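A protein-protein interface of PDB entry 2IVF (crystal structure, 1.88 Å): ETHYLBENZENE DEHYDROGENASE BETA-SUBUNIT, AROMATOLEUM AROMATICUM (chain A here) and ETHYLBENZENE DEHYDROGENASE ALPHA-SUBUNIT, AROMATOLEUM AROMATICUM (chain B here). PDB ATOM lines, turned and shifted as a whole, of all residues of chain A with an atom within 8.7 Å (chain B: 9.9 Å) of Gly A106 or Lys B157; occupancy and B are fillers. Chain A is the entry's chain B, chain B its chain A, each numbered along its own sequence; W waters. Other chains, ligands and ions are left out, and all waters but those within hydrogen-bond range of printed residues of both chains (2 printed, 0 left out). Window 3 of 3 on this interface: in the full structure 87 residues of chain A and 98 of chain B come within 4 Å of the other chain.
The side-chain carboxylate of Glu A101 is in salt-bridge range of the side-chain amino group of Lys A107 (2.7 Å).
OE2 of Glu B155 is in salt-bridge range of NZ of Lys B157 (3.8 Å).
O of Lys B157 sits at hydrogen-bond distance from N of Val B150 (2.9 Å).
OE1 of Glu B155 lies within hydrogen-bond range of N of Lys B152 (2.9 Å).
The side-chain hydroxyl (OG1) of Thr A110 sits at hydrogen-bond distance from the backbone carbonyl oxygen (O) of Lys A107 (2.6 Å).
The backbone NH of Gly B154 sits at hydrogen-bond distance from the backbone carbonyl oxygen of Met B644 (3.0 Å).
Water W2 lies within hydrogen-bond range of the backbone carbonyl oxygen of Tyr A104 (2.7 Å) and the backbone NH of Trp B158 (2.8 Å).
Water W1 lies within hydrogen-bond range of OE1 of Gln A109 (3.1 Å) and O of Gly B154 (3.5 Å).
Of the printed residues of chain B, Glu A105 touches Gly B156 (3.3 Å).
Of chain B, only Glu B155 (3.1 Å), Gly B156 (2.8 Å) and Lys B157 (3.5 Å) come within 4 Å of Gly A106.
Of the printed residues of chain A, Glu B155 touches Gly A106 (3.1 Å), Lys A107 (3.4 Å) and Gly A108 (2.9 Å).
Gly B156 touches four residues of chain A.
Lys B157 touches just one residue of chain A: Gly A106 (3.5 Å).
Of the printed residues of chain A, Trp B929 touches Val A102, Gly A108, Gln A109 and Val A111.
The nearest printed residue of chain B that does not touch Tyr A104 is Met B639 (4.05 Å).
NE2 of Gln A109 is in hydrogen-bond range of O of Gly B154 (2.8 Å).
The backbone NH (N) of Lys A107 is in hydrogen-bond range of the backbone carbonyl oxygen (O) of Glu B155.
The backbone carbonyl oxygen (O) of Phe A103 sits close to the indole nitrogen (NE1) of Trp B158 (3.1 Å).
The backbone NH of Gly A108 lies within hydrogen-bond range of the backbone carbonyl oxygen of Glu B155, at 2.9 Å.
The backbone carbonyl oxygen (O) of Gly B156 lies within hydrogen-bond range of the backbone NH (N) of Gly A106, 2.8 Å away.
O of Phe A103 sits close to O of Gly B156, at 3.5 Å.
The backbone carbonyl oxygen (O) of Gly B156 is in hydrogen-bond range of the backbone NH (N) of Glu A105 (3.3 Å).
NE1 of Trp B929 lies within hydrogen-bond range of O of Val A111 (2.8 Å).
The backbone carbonyl oxygen (O) of Phe A103 sits close to the side-chain sulfur (SD) of Met B644 (3.7 Å).
O of Tyr A104 lies close to O of Gly B156 (3.2 Å).
Among the printed residues, pairs that only touch across the chains: Val A102 with Met B644 (3.2 Å), Val A102 with Trp B929 (3.96 Å), Phe A103 with Met B639 (3.5 Å), Tyr A104 with Trp B158 (3.7 Å), Gly A106 with Glu B155 (3.1 Å), Gly A106 with Lys B157 (3.5 Å), Gly A108 with Gly B154 (3.4 Å), Gly A108 with Trp B929 (3.6 Å), Gln A109 with Tyr B645 (3.6 Å) and Gln A109 with Trp B929 (3.4 Å).
Of the 12 printed residues of chain A, 9 touch a printed residue of chain B.
Hydrophobic or aromatic side chains of chain A within 4 Å of the printed part of chain B: Val A102, Phe A103 and Tyr A104.
Among the printed residues, no Asp or Glu carboxylate lies within 4 Å of a Lys or Arg side-chain nitrogen of the other chain.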
ATOM      1  N   LYS A 100     -18.571 -17.244 -16.244  1.00  0.00           N
ATOM      2  CA  LYS A 100     -19.871 -16.622 -15.925  1.00  0.00           C
ATOM      3  C   LYS A 100     -20.163 -15.432 -16.837  1.00  0.00           C
ATOM      4  O   LYS A 100     -21.247 -15.321 -17.390  1.00  0.00           O
ATOM      5  CB  LYS A 100     -19.960 -16.149 -14.449  1.00  0.00           C
ATOM      6  CG  LYS A 100     -21.399 -15.738 -14.010  1.00  0.00           C
ATOM      7  CD  LYS A 100     -21.502 -15.289 -12.515  1.00  0.00           C
ATOM      8  CE  LYS A 100     -22.706 -14.439 -12.249  1.00  0.00           C
ATOM      9  NZ  LYS A 100     -22.797 -13.974 -10.792  1.00  0.00           N
ATOM     10  N   GLU A 101     -19.162 -14.569 -17.014  1.00  0.00           N
ATOM     11  CA  GLU A 101     -19.301 -13.357 -17.810  1.00  0.00           C
ATOM     12  C   GLU A 101     -19.709 -13.660 -19.252  1.00  0.00           C
ATOM     13  O   GLU A 101     -20.562 -12.990 -19.831  1.00  0.00           O
ATOM     14  CB  GLU A 101     -17.972 -12.576 -17.811  1.00  0.00           C
ATOM     15  CG  GLU A 101     -18.113 -11.224 -18.385  1.00  0.00           C
ATOM     16  CD  GLU A 101     -16.851 -10.412 -18.329  1.00  0.00           C
ATOM     17  OE1 GLU A 101     -15.753 -10.966 -18.514  1.00  0.00           O
ATOM     18  OE2 GLU A 101     -16.991  -9.180 -18.135  1.00  0.00           O
ATOM     19  N   VAL A 102     -19.069 -14.667 -19.827  1.00  0.00           N
ATOM     20  CA  VAL A 102     -19.322 -15.065 -21.216  1.00  0.00           C
ATOM     21  C   VAL A 102     -20.665 -15.817 -21.387  1.00  0.00           C
ATOM     22  O   VAL A 102     -21.386 -15.605 -22.366  1.00  0.00           O
ATOM     23  CB  VAL A 102     -18.156 -15.876 -21.763  1.00  0.00           C
ATOM     24  CG1 VAL A 102     -18.467 -16.338 -23.189  1.00  0.00           C
ATOM     25  CG2 VAL A 102     -16.870 -15.058 -21.705  1.00  0.00           C
ATOM     26  N   PHE A 103     -21.050 -16.652 -20.415  1.00  0.00           N
ATOM     27  CA  PHE A 103     -22.216 -17.536 -20.628  1.00  0.00           C
ATOM     28  C   PHE A 103     -23.539 -17.020 -20.125  1.00  0.00           C
ATOM     29  O   PHE A 103     -24.591 -17.354 -20.671  1.00  0.00           O
ATOM     30  CB  PHE A 103     -21.945 -18.894 -19.952  1.00  0.00           C
ATOM     31  CG  PHE A 103     -20.643 -19.529 -20.331  1.00  0.00           C
ATOM     32  CD1 PHE A 103     -20.051 -19.314 -21.578  1.00  0.00           C
ATOM     33  CD2 PHE A 103     -20.026 -20.418 -19.460  1.00  0.00           C
ATOM     34  CE1 PHE A 103     -18.874 -19.952 -21.924  1.00  0.00           C
ATOM     35  CE2 PHE A 103     -18.827 -21.042 -19.807  1.00  0.00           C
ATOM     36  CZ  PHE A 103     -18.238 -20.807 -21.027  1.00  0.00           C
ATOM     37  N   TYR A 104     -23.511 -16.244 -19.045  1.00  0.00           N
ATOM     38  CA  TYR A 104     -24.704 -16.053 -18.234  1.00  0.00           C
ATOM     39  C   TYR A 104     -25.075 -14.610 -17.949  1.00  0.00           C
ATOM     40  O   TYR A 104     -26.121 -14.370 -17.326  1.00  0.00           O
ATOM     41  CB  TYR A 104     -24.504 -16.766 -16.885  1.00  0.00           C
ATOM     42  CG  TYR A 104     -24.194 -18.233 -17.040  1.00  0.00           C
ATOM     43  CD1 TYR A 104     -25.056 -19.052 -17.751  1.00  0.00           C
ATOM     44  CD2 TYR A 104     -23.092 -18.803 -16.449  1.00  0.00           C
ATOM     45  CE1 TYR A 104     -24.808 -20.367 -17.907  1.00  0.00           C
ATOM     46  CE2 TYR A 104     -22.823 -20.149 -16.610  1.00  0.00           C
ATOM     47  CZ  TYR A 104     -23.721 -20.925 -17.345  1.00  0.00           C
ATOM     48  OH  TYR A 104     -23.507 -22.261 -17.539  1.00  0.00           O
ATOM     49  N   GLU A 105     -24.251 -13.659 -18.373  1.00  0.00           N
ATOM     50  CA  GLU A 105     -24.421 -12.286 -17.917  1.00  0.00           C
ATOM     51  C   GLU A 105     -25.146 -11.404 -18.901  1.00  0.00           C
ATOM     52  O   GLU A 105     -25.337 -10.216 -18.654  1.00  0.00           O
ATOM     53  CB  GLU A 105     -23.091 -11.695 -17.423  1.00  0.00           C
ATOM     54  CG  GLU A 105     -22.773 -12.189 -15.998  1.00  0.00           C
ATOM     55  CD  GLU A 105     -21.468 -11.665 -15.438  1.00  0.00           C
ATOM     56  OE1 GLU A 105     -20.933 -10.679 -15.980  1.00  0.00           O
ATOM     57  OE2 GLU A 105     -20.968 -12.255 -14.445  1.00  0.00           O
ATOM     58  N   GLY A 106     -25.659 -11.986 -19.969  1.00  0.00           N
ATOM     59  CA  GLY A 106     -26.457 -11.225 -20.920  1.00  0.00           C
ATOM     60  C   GLY A 106     -25.631 -10.199 -21.710  1.00  0.00           C
ATOM     61  O   GLY A 106     -26.183  -9.205 -22.219  1.00  0.00           O
ATOM     62  N   LYS A 107     -24.326 -10.443 -21.821  1.00  0.00           N
ATOM     63  CA  LYS A 107     -23.410  -9.530 -22.502  1.00  0.00           C
ATOM     64  C   LYS A 107     -23.223  -9.895 -23.970  1.00  0.00           C
ATOM     65  O   LYS A 107     -22.524  -9.184 -24.709  1.00  0.00           O
ATOM     66  CB  LYS A 107     -22.051  -9.472 -21.770  1.00  0.00           C
ATOM     67  CG  LYS A 107     -22.142  -8.870 -20.373  1.00  0.00           C
ATOM     68  CD  LYS A 107     -20.749  -8.841 -19.716  1.00  0.00           C
ATOM     69  CE  LYS A 107     -20.691  -7.915 -18.504  1.00  0.00           C
ATOM     70  NZ  LYS A 107     -19.232  -7.767 -18.066  1.00  0.00           N
ATOM     71  N   GLY A 108     -23.871 -10.978 -24.413  1.00  0.00           N
ATOM     72  CA  GLY A 108     -23.827 -11.369 -25.810  1.00  0.00           C
ATOM     73  C   GLY A 108     -22.411 -11.565 -26.308  1.00  0.00           C
ATOM     74  O   GLY A 108     -21.541 -12.097 -25.577  1.00  0.00           O
ATOM     75  N   GLN A 109     -22.142 -11.067 -27.516  1.00  0.00           N
ATOM     76  CA  GLN A 109     -20.806 -11.171 -28.098  1.00  0.00           C
ATOM     77  C   GLN A 109     -19.862 -10.017 -27.702  1.00  0.00           C
ATOM     78  O   GLN A 109     -18.777  -9.908 -28.256  1.00  0.00           O
ATOM     79  CB  GLN A 109     -20.904 -11.263 -29.625  1.00  0.00           C
ATOM     80  CG  GLN A 109     -21.408 -12.603 -30.130  1.00  0.00           C
ATOM     81  CD  GLN A 109     -22.829 -12.866 -29.701  1.00  0.00           C
ATOM     82  OE1 GLN A 109     -23.719 -12.135 -30.071  1.00  0.00           O
ATOM     83  NE2 GLN A 109     -23.038 -13.911 -28.907  1.00  0.00           N
ATOM     84  N   THR A 110     -20.248  -9.209 -26.732  1.00  0.00           N
ATOM     85  CA  THR A 110     -19.431  -8.065 -26.305  1.00  0.00           C
ATOM     86  C   THR A 110     -18.306  -8.448 -25.378  1.00  0.00           C
ATOM     87  O   THR A 110     -17.485  -7.603 -25.019  1.00  0.00           O
ATOM     88  CB  THR A 110     -20.267  -6.968 -25.661  1.00  0.00           C
ATOM     89  OG1 THR A 110     -20.696  -7.347 -24.339  1.00  0.00           O
ATOM     90  CG2 THR A 110     -21.438  -6.631 -26.578  1.00  0.00           C
ATOM     91  N   VAL A 111     -18.293  -9.717 -24.969  1.00  0.00           N
ATOM     92  CA  VAL A 111     -17.245 -10.240 -24.149  1.00  0.00           C
ATOM     93  C   VAL A 111     -16.927 -11.609 -24.735  1.00  0.00           C
ATOM     94  O   VAL A 111     -17.721 -12.177 -25.464  1.00  0.00           O
ATOM     95  CB  VAL A 111     -17.687 -10.320 -22.671  1.00  0.00           C
ATOM     96  CG1 VAL A 111     -18.158  -8.914 -22.173  1.00  0.00           C
ATOM     97  CG2 VAL A 111     -18.827 -11.360 -22.473  1.00  0.00           C
ATOM     98  N   LEU B 147     -31.250 -25.461 -19.262  1.00  0.00           N
ATOM     99  CA  LEU B 147     -31.355 -24.018 -19.422  1.00  0.00           C
ATOM    100  C   LEU B 147     -32.261 -23.712 -20.572  1.00  0.00           C
ATOM    101  O   LEU B 147     -32.186 -24.379 -21.622  1.00  0.00           O
ATOM    102  CB  LEU B 147     -29.971 -23.469 -19.740  1.00  0.00           C
ATOM    103  CG  LEU B 147     -28.960 -23.674 -18.621  1.00  0.00           C
ATOM    104  CD1 LEU B 147     -27.529 -23.232 -19.121  1.00  0.00           C
ATOM    105  CD2 LEU B 147     -29.423 -22.936 -17.378  1.00  0.00           C
ATOM    106  N   LYS B 148     -33.041 -22.658 -20.402  1.00  0.00           N
ATOM    107  CA  LYS B 148     -33.892 -22.145 -21.436  1.00  0.00           C
ATOM    108  C   LYS B 148     -33.536 -20.683 -21.735  1.00  0.00           C
ATOM    109  O   LYS B 148     -33.381 -19.867 -20.836  1.00  0.00           O
ATOM    110  CB  LYS B 148     -35.346 -22.272 -21.007  1.00  0.00           C
ATOM    111  CG  LYS B 148     -36.350 -21.649 -21.996  1.00  0.00           C
ATOM    112  CD  LYS B 148     -37.709 -22.244 -21.713  1.00  0.00           C
ATOM    113  CE  LYS B 148     -38.799 -21.705 -22.551  1.00  0.00           C
ATOM    114  NZ  LYS B 148     -39.923 -22.704 -22.455  1.00  0.00           N
ATOM    115  N   ARG B 149     -33.455 -20.375 -23.016  1.00  0.00           N
ATOM    116  CA  ARG B 149     -33.123 -19.056 -23.478  1.00  0.00           C
ATOM    117  C   ARG B 149     -34.137 -18.039 -23.001  1.00  0.00           C
ATOM    118  O   ARG B 149     -35.354 -18.238 -23.102  1.00  0.00           O
ATOM    119  CB  ARG B 149     -33.098 -19.036 -25.014  1.00  0.00           C
ATOM    120  CG  ARG B 149     -32.933 -17.676 -25.616  1.00  0.00           C
ATOM    121  CD  ARG B 149     -32.667 -17.791 -27.118  1.00  0.00           C
ATOM    122  NE  ARG B 149     -33.815 -18.336 -27.872  1.00  0.00           N
ATOM    123  CZ  ARG B 149     -34.852 -17.647 -28.341  1.00  0.00           C
ATOM    124  NH1 ARG B 149     -34.990 -16.338 -28.116  1.00  0.00           N
ATOM    125  NH2 ARG B 149     -35.801 -18.286 -29.022  1.00  0.00           N
ATOM    126  N   VAL B 150     -33.598 -16.922 -22.526  1.00  0.00           N
ATOM    127  CA  VAL B 150     -34.372 -15.803 -22.099  1.00  0.00           C
ATOM    128  C   VAL B 150     -34.304 -14.609 -23.049  1.00  0.00           C
ATOM    129  O   VAL B 150     -35.325 -13.986 -23.300  1.00  0.00           O
ATOM    130  CB  VAL B 150     -33.955 -15.393 -20.671  1.00  0.00           C
ATOM    131  CG1 VAL B 150     -34.525 -14.010 -20.310  1.00  0.00           C
ATOM    132  CG2 VAL B 150     -34.494 -16.430 -19.692  1.00  0.00           C
ATOM    133  N   GLY B 151     -33.112 -14.284 -23.544  1.00  0.00           N
ATOM    134  CA  GLY B 151     -32.958 -13.169 -24.483  1.00  0.00           C
ATOM    135  C   GLY B 151     -33.001 -13.675 -25.918  1.00  0.00           C
ATOM    136  O   GLY B 151     -33.722 -14.635 -26.230  1.00  0.00           O
ATOM    137  N   LYS B 152     -32.249 -13.015 -26.786  1.00  0.00           N
ATOM    138  CA  LYS B 152     -32.076 -13.440 -28.169  1.00  0.00           C
ATOM    139  C   LYS B 152     -31.110 -14.582 -28.165  1.00  0.00           C
ATOM    140  O   LYS B 152     -30.364 -14.772 -27.201  1.00  0.00           O
ATOM    141  CB  LYS B 152     -31.446 -12.325 -29.001  1.00  0.00           C
ATOM    142  CG  LYS B 152     -32.192 -11.052 -29.064  1.00  0.00           C
ATOM    143  CD  LYS B 152     -33.555 -11.222 -29.665  1.00  0.00           C
ATOM    144  CE  LYS B 152     -34.141  -9.875 -30.075  1.00  0.00           C
ATOM    145  NZ  LYS B 152     -35.604  -9.924 -30.415  1.00  0.00           N
ATOM    146  N   ARG B 153     -31.091 -15.353 -29.243  1.00  0.00           N
ATOM    147  CA  ARG B 153     -30.067 -16.385 -29.373  1.00  0.00           C
ATOM    148  C   ARG B 153     -28.678 -15.773 -29.320  1.00  0.00           C
ATOM    149  O   ARG B 153     -28.375 -14.812 -30.063  1.00  0.00           O
ATOM    150  CB  ARG B 153     -30.257 -17.189 -30.657  1.00  0.00           C
ATOM    151  CG  ARG B 153     -31.513 -18.072 -30.642  1.00  0.00           C
ATOM    152  CD  ARG B 153     -31.873 -18.631 -32.015  1.00  0.00           C
ATOM    153  NE  ARG B 153     -32.941 -19.633 -31.921  1.00  0.00           N
ATOM    154  CZ  ARG B 153     -33.689 -20.052 -32.939  1.00  0.00           C
ATOM    155  NH1 ARG B 153     -33.534 -19.556 -34.167  1.00  0.00           N
ATOM    156  NH2 ARG B 153     -34.613 -20.955 -32.722  1.00  0.00           N
ATOM    157  N   GLY B 154     -27.850 -16.306 -28.429  1.00  0.00           N
ATOM    158  CA  GLY B 154     -26.489 -15.820 -28.272  1.00  0.00           C
ATOM    159  C   GLY B 154     -26.301 -14.657 -27.321  1.00  0.00           C
ATOM    160  O   GLY B 154     -25.191 -14.167 -27.174  1.00  0.00           O
ATOM    161  N   GLU B 155     -27.374 -14.173 -26.702  1.00  0.00           N
ATOM    162  CA  GLU B 155     -27.283 -12.993 -25.856  1.00  0.00           C
ATOM    163  C   GLU B 155     -26.700 -13.279 -24.485  1.00  0.00           C
ATOM    164  O   GLU B 155     -26.299 -12.347 -23.772  1.00  0.00           O
ATOM    165  CB  GLU B 155     -28.665 -12.364 -25.712  1.00  0.00           C
ATOM    166  CG  GLU B 155     -28.582 -10.998 -25.135  1.00  0.00           C
ATOM    167  CD  GLU B 155     -29.857 -10.216 -25.255  1.00  0.00           C
ATOM    168  OE1 GLU B 155     -30.923 -10.802 -25.560  1.00  0.00           O
ATOM    169  OE2 GLU B 155     -29.763  -9.007 -24.995  1.00  0.00           O
ATOM    170  N   GLY B 156     -26.728 -14.555 -24.083  1.00  0.00           N
ATOM    171  CA  GLY B 156     -26.157 -14.999 -22.810  1.00  0.00           C
ATOM    172  C   GLY B 156     -27.083 -14.786 -21.637  1.00  0.00           C
ATOM    173  O   GLY B 156     -26.635 -14.522 -20.498  1.00  0.00           O
ATOM    174  N   LYS B 157     -28.381 -14.855 -21.928  1.00  0.00           N
ATOM    175  CA  LYS B 157     -29.415 -14.760 -20.917  1.00  0.00           C
ATOM    176  C   LYS B 157     -30.174 -16.090 -20.852  1.00  0.00           C
ATOM    177  O   LYS B 157     -30.853 -16.497 -21.822  1.00  0.00           O
ATOM    178  CB  LYS B 157     -30.389 -13.606 -21.219  1.00  0.00           C
ATOM    179  CG  LYS B 157     -29.768 -12.191 -21.283  1.00  0.00           C
ATOM    180  CD  LYS B 157     -30.875 -11.130 -21.378  1.00  0.00           C
ATOM    181  CE  LYS B 157     -30.317  -9.716 -21.493  1.00  0.00           C
ATOM    182  NZ  LYS B 157     -31.397  -8.714 -21.524  1.00  0.00           N
ATOM    183  N   TRP B 158     -30.030 -16.776 -19.711  1.00  0.00           N
ATOM    184  CA  TRP B 158     -30.579 -18.090 -19.506  1.00  0.00           C
ATOM    185  C   TRP B 158     -31.336 -18.199 -18.194  1.00  0.00           C
ATOM    186  O   TRP B 158     -31.101 -17.459 -17.230  1.00  0.00           O
ATOM    187  CB  TRP B 158     -29.414 -19.083 -19.419  1.00  0.00           C
ATOM    188  CG  TRP B 158     -28.537 -19.191 -20.612  1.00  0.00           C
ATOM    189  CD1 TRP B 158     -27.255 -18.720 -20.756  1.00  0.00           C
ATOM    190  CD2 TRP B 158     -28.839 -19.906 -21.815  1.00  0.00           C
ATOM    191  NE1 TRP B 158     -26.755 -19.092 -21.990  1.00  0.00           N
ATOM    192  CE2 TRP B 158     -27.706 -19.828 -22.650  1.00  0.00           C
ATOM    193  CE3 TRP B 158     -29.959 -20.624 -22.258  1.00  0.00           C
ATOM    194  CZ2 TRP B 158     -27.665 -20.427 -23.880  1.00  0.00           C
ATOM    195  CZ3 TRP B 158     -29.924 -21.207 -23.500  1.00  0.00           C
ATOM    196  CH2 TRP B 158     -28.782 -21.114 -24.297  1.00  0.00           C
ATOM    197  N   LYS B 159     -32.284 -19.124 -18.160  1.00  0.00           N
ATOM    198  CA  LYS B 159     -32.917 -19.533 -16.912  1.00  0.00           C
ATOM    199  C   LYS B 159     -32.963 -21.051 -16.824  1.00  0.00           C
ATOM    200  O   LYS B 159     -33.008 -21.767 -17.839  1.00  0.00           O
ATOM    201  CB  LYS B 159     -34.314 -18.944 -16.816  1.00  0.00           C
ATOM    202  CG  LYS B 159     -35.392 -19.673 -17.606  1.00  0.00           C
ATOM    203  CD  LYS B 159     -36.697 -18.900 -17.528  1.00  0.00           C
ATOM    204  CE  LYS B 159     -37.738 -19.417 -18.509  1.00  0.00           C
ATOM    205  NZ  LYS B 159     -39.014 -18.674 -18.403  1.00  0.00           N
ATOM    206  N   ARG B 160     -32.857 -21.537 -15.600  1.00  0.00           N
ATOM    207  CA  ARG B 160     -32.971 -22.936 -15.341  1.00  0.00           C
ATOM    208  C   ARG B 160     -34.434 -23.326 -15.520  1.00  0.00           C
ATOM    209  O   ARG B 160     -35.324 -22.601 -15.090  1.00  0.00           O
ATOM    210  CB  ARG B 160     -32.607 -23.173 -13.892  1.00  0.00           C
ATOM    211  CG  ARG B 160     -32.688 -24.603 -13.453  1.00  0.00           C
ATOM    212  CD  ARG B 160     -32.476 -24.688 -11.951  1.00  0.00           C
ATOM    213  NE  ARG B 160     -32.611 -26.072 -11.479  1.00  0.00           N
ATOM    214  CZ  ARG B 160     -32.473 -26.454 -10.204  1.00  0.00           C
ATOM    215  NH1 ARG B 160     -32.170 -25.570  -9.247  1.00  0.00           N
ATOM    216  NH2 ARG B 160     -32.629 -27.737  -9.879  1.00  0.00           N
ATOM    217  N   MET B 639     -20.663 -25.317 -22.004  1.00  0.00           N
ATOM    218  CA  MET B 639     -21.267 -24.188 -22.703  1.00  0.00           C
ATOM    219  C   MET B 639     -20.409 -23.833 -23.915  1.00  0.00           C
ATOM    220  O   MET B 639     -19.516 -22.970 -23.866  1.00  0.00           O
ATOM    221  CB  MET B 639     -21.514 -22.990 -21.804  1.00  0.00           C
ATOM    222  CG  MET B 639     -22.244 -21.900 -22.530  1.00  0.00           C
ATOM    223  SD  MET B 639     -23.920 -22.367 -23.017  1.00  0.00           S
ATOM    224  CE  MET B 639     -24.820 -22.255 -21.486  1.00  0.00           C
ATOM    225  N   ALA B 643     -23.856 -23.797 -28.380  1.00  0.00           N
ATOM    226  CA  ALA B 643     -24.877 -23.899 -27.336  1.00  0.00           C
ATOM    227  C   ALA B 643     -25.354 -22.537 -26.872  1.00  0.00           C
ATOM    228  O   ALA B 643     -26.495 -22.386 -26.453  1.00  0.00           O
ATOM    229  CB  ALA B 643     -24.345 -24.741 -26.118  1.00  0.00           C
ATOM    230  N   MET B 644     -24.477 -21.532 -26.943  1.00  0.00           N
ATOM    231  CA  MET B 644     -24.861 -20.165 -26.608  1.00  0.00           C
ATOM    232  C   MET B 644     -25.972 -19.632 -27.487  1.00  0.00           C
ATOM    233  O   MET B 644     -26.653 -18.686 -27.117  1.00  0.00           O
ATOM    234  CB  MET B 644     -23.636 -19.254 -26.604  1.00  0.00           C
ATOM    235  CG  MET B 644     -22.755 -19.521 -25.367  1.00  0.00           C
ATOM    236  SD  MET B 644     -23.577 -19.008 -23.847  1.00  0.00           S
ATOM    237  CE  MET B 644     -23.632 -17.208 -24.014  1.00  0.00           C
ATOM    238  N   TYR B 645     -26.161 -20.231 -28.658  1.00  0.00           N
ATOM    239  CA  TYR B 645     -27.225 -19.822 -29.557  1.00  0.00           C
ATOM    240  C   TYR B 645     -28.442 -20.717 -29.501  1.00  0.00           C
ATOM    241  O   TYR B 645     -29.412 -20.493 -30.218  1.00  0.00           O
ATOM    242  CB  TYR B 645     -26.721 -19.814 -30.998  1.00  0.00           C
ATOM    243  CG  TYR B 645     -25.714 -18.763 -31.249  1.00  0.00           C
ATOM    244  CD1 TYR B 645     -24.393 -19.002 -30.963  1.00  0.00           C
ATOM    245  CD2 TYR B 645     -26.076 -17.498 -31.744  1.00  0.00           C
ATOM    246  CE1 TYR B 645     -23.447 -18.048 -31.171  1.00  0.00           C
ATOM    247  CE2 TYR B 645     -25.094 -16.526 -31.967  1.00  0.00           C
ATOM    248  CZ  TYR B 645     -23.775 -16.849 -31.671  1.00  0.00           C
ATOM    249  OH  TYR B 645     -22.724 -15.955 -31.851  1.00  0.00           O
ATOM    250  N   ALA B 646     -28.417 -21.700 -28.627  1.00  0.00           N
ATOM    251  CA  ALA B 646     -29.518 -22.629 -28.512  1.00  0.00           C
ATOM    252  C   ALA B 646     -30.707 -22.015 -27.788  1.00  0.00           C
ATOM    253  O   ALA B 646     -30.600 -21.015 -27.054  1.00  0.00           O
ATOM    254  CB  ALA B 646     -29.048 -23.884 -27.761  1.00  0.00           C
ATOM    255  N   ASP B 647     -31.863 -22.618 -27.999  1.00  0.00           N
ATOM    256  CA  ASP B 647     -33.048 -22.284 -27.269  1.00  0.00           C
ATOM    257  C   ASP B 647     -33.120 -23.050 -25.982  1.00  0.00           C
ATOM    258  O   ASP B 647     -33.657 -22.541 -25.015  1.00  0.00           O
ATOM    259  CB  ASP B 647     -34.270 -22.580 -28.112  1.00  0.00           C
ATOM    260  CG  ASP B 647     -34.214 -21.880 -29.439  1.00  0.00           C
ATOM    261  OD1 ASP B 647     -33.935 -20.650 -29.472  1.00  0.00           O
ATOM    262  OD2 ASP B 647     -34.439 -22.568 -30.444  1.00  0.00           O
ATOM    263  N   ILE B 648     -32.588 -24.274 -25.990  1.00  0.00           N
ATOM    264  CA  ILE B 648     -32.654 -25.183 -24.860  1.00  0.00           C
ATOM    265  C   ILE B 648     -31.303 -25.884 -24.772  1.00  0.00           C
ATOM    266  O   ILE B 648     -30.784 -26.385 -25.775  1.00  0.00           O
ATOM    267  CB  ILE B 648     -33.772 -26.264 -25.063  1.00  0.00           C
ATOM    268  CG1 ILE B 648     -35.167 -25.660 -25.095  1.00  0.00           C
ATOM    269  CG2 ILE B 648     -33.687 -27.340 -23.963  1.00  0.00           C
ATOM    270  CD1 ILE B 648     -35.628 -24.994 -23.804  1.00  0.00           C
ATOM    271  N   VAL B 649     -30.714 -25.918 -23.583  1.00  0.00           N
ATOM    272  CA  VAL B 649     -29.504 -26.682 -23.368  1.00  0.00           C
ATOM    273  C   VAL B 649     -29.813 -27.711 -22.287  1.00  0.00           C
ATOM    274  O   VAL B 649     -30.305 -27.351 -21.194  1.00  0.00           O
ATOM    275  CB  VAL B 649     -28.335 -25.774 -22.965  1.00  0.00           C
ATOM    276  CG1 VAL B 649     -27.066 -26.604 -22.701  1.00  0.00           C
ATOM    277  CG2 VAL B 649     -28.089 -24.698 -24.055  1.00  0.00           C
ATOM    278  N   TRP B 929     -16.782 -13.107 -30.985  1.00  0.00           N
ATOM    279  CA  TRP B 929     -17.029 -14.520 -31.299  1.00  0.00           C
ATOM    280  C   TRP B 929     -16.911 -14.836 -32.796  1.00  0.00           C
ATOM    281  O   TRP B 929     -17.633 -15.698 -33.331  1.00  0.00           O
ATOM    282  CB  TRP B 929     -18.410 -14.994 -30.834  1.00  0.00           C
ATOM    283  CG  TRP B 929     -18.691 -14.833 -29.410  1.00  0.00           C
ATOM    284  CD1 TRP B 929     -18.084 -14.014 -28.526  1.00  0.00           C
ATOM    285  CD2 TRP B 929     -19.762 -15.461 -28.713  1.00  0.00           C
ATOM    286  NE1 TRP B 929     -18.673 -14.141 -27.285  1.00  0.00           N
ATOM    287  CE2 TRP B 929     -19.708 -15.023 -27.381  1.00  0.00           C
ATOM    288  CE3 TRP B 929     -20.720 -16.406 -29.076  1.00  0.00           C
ATOM    289  CZ2 TRP B 929     -20.616 -15.462 -26.403  1.00  0.00           C
ATOM    290  CZ3 TRP B 929     -21.618 -16.847 -28.108  1.00  0.00           C
ATOM    291  CH2 TRP B 929     -21.547 -16.379 -26.790  1.00  0.00           C
HETATM  292  O   HOH W   1     -26.647 -11.781 -29.210  1.00  0.00           O
HETATM  293  O   HOH W   2     -28.138 -16.110 -17.725  1.00  0.00           O
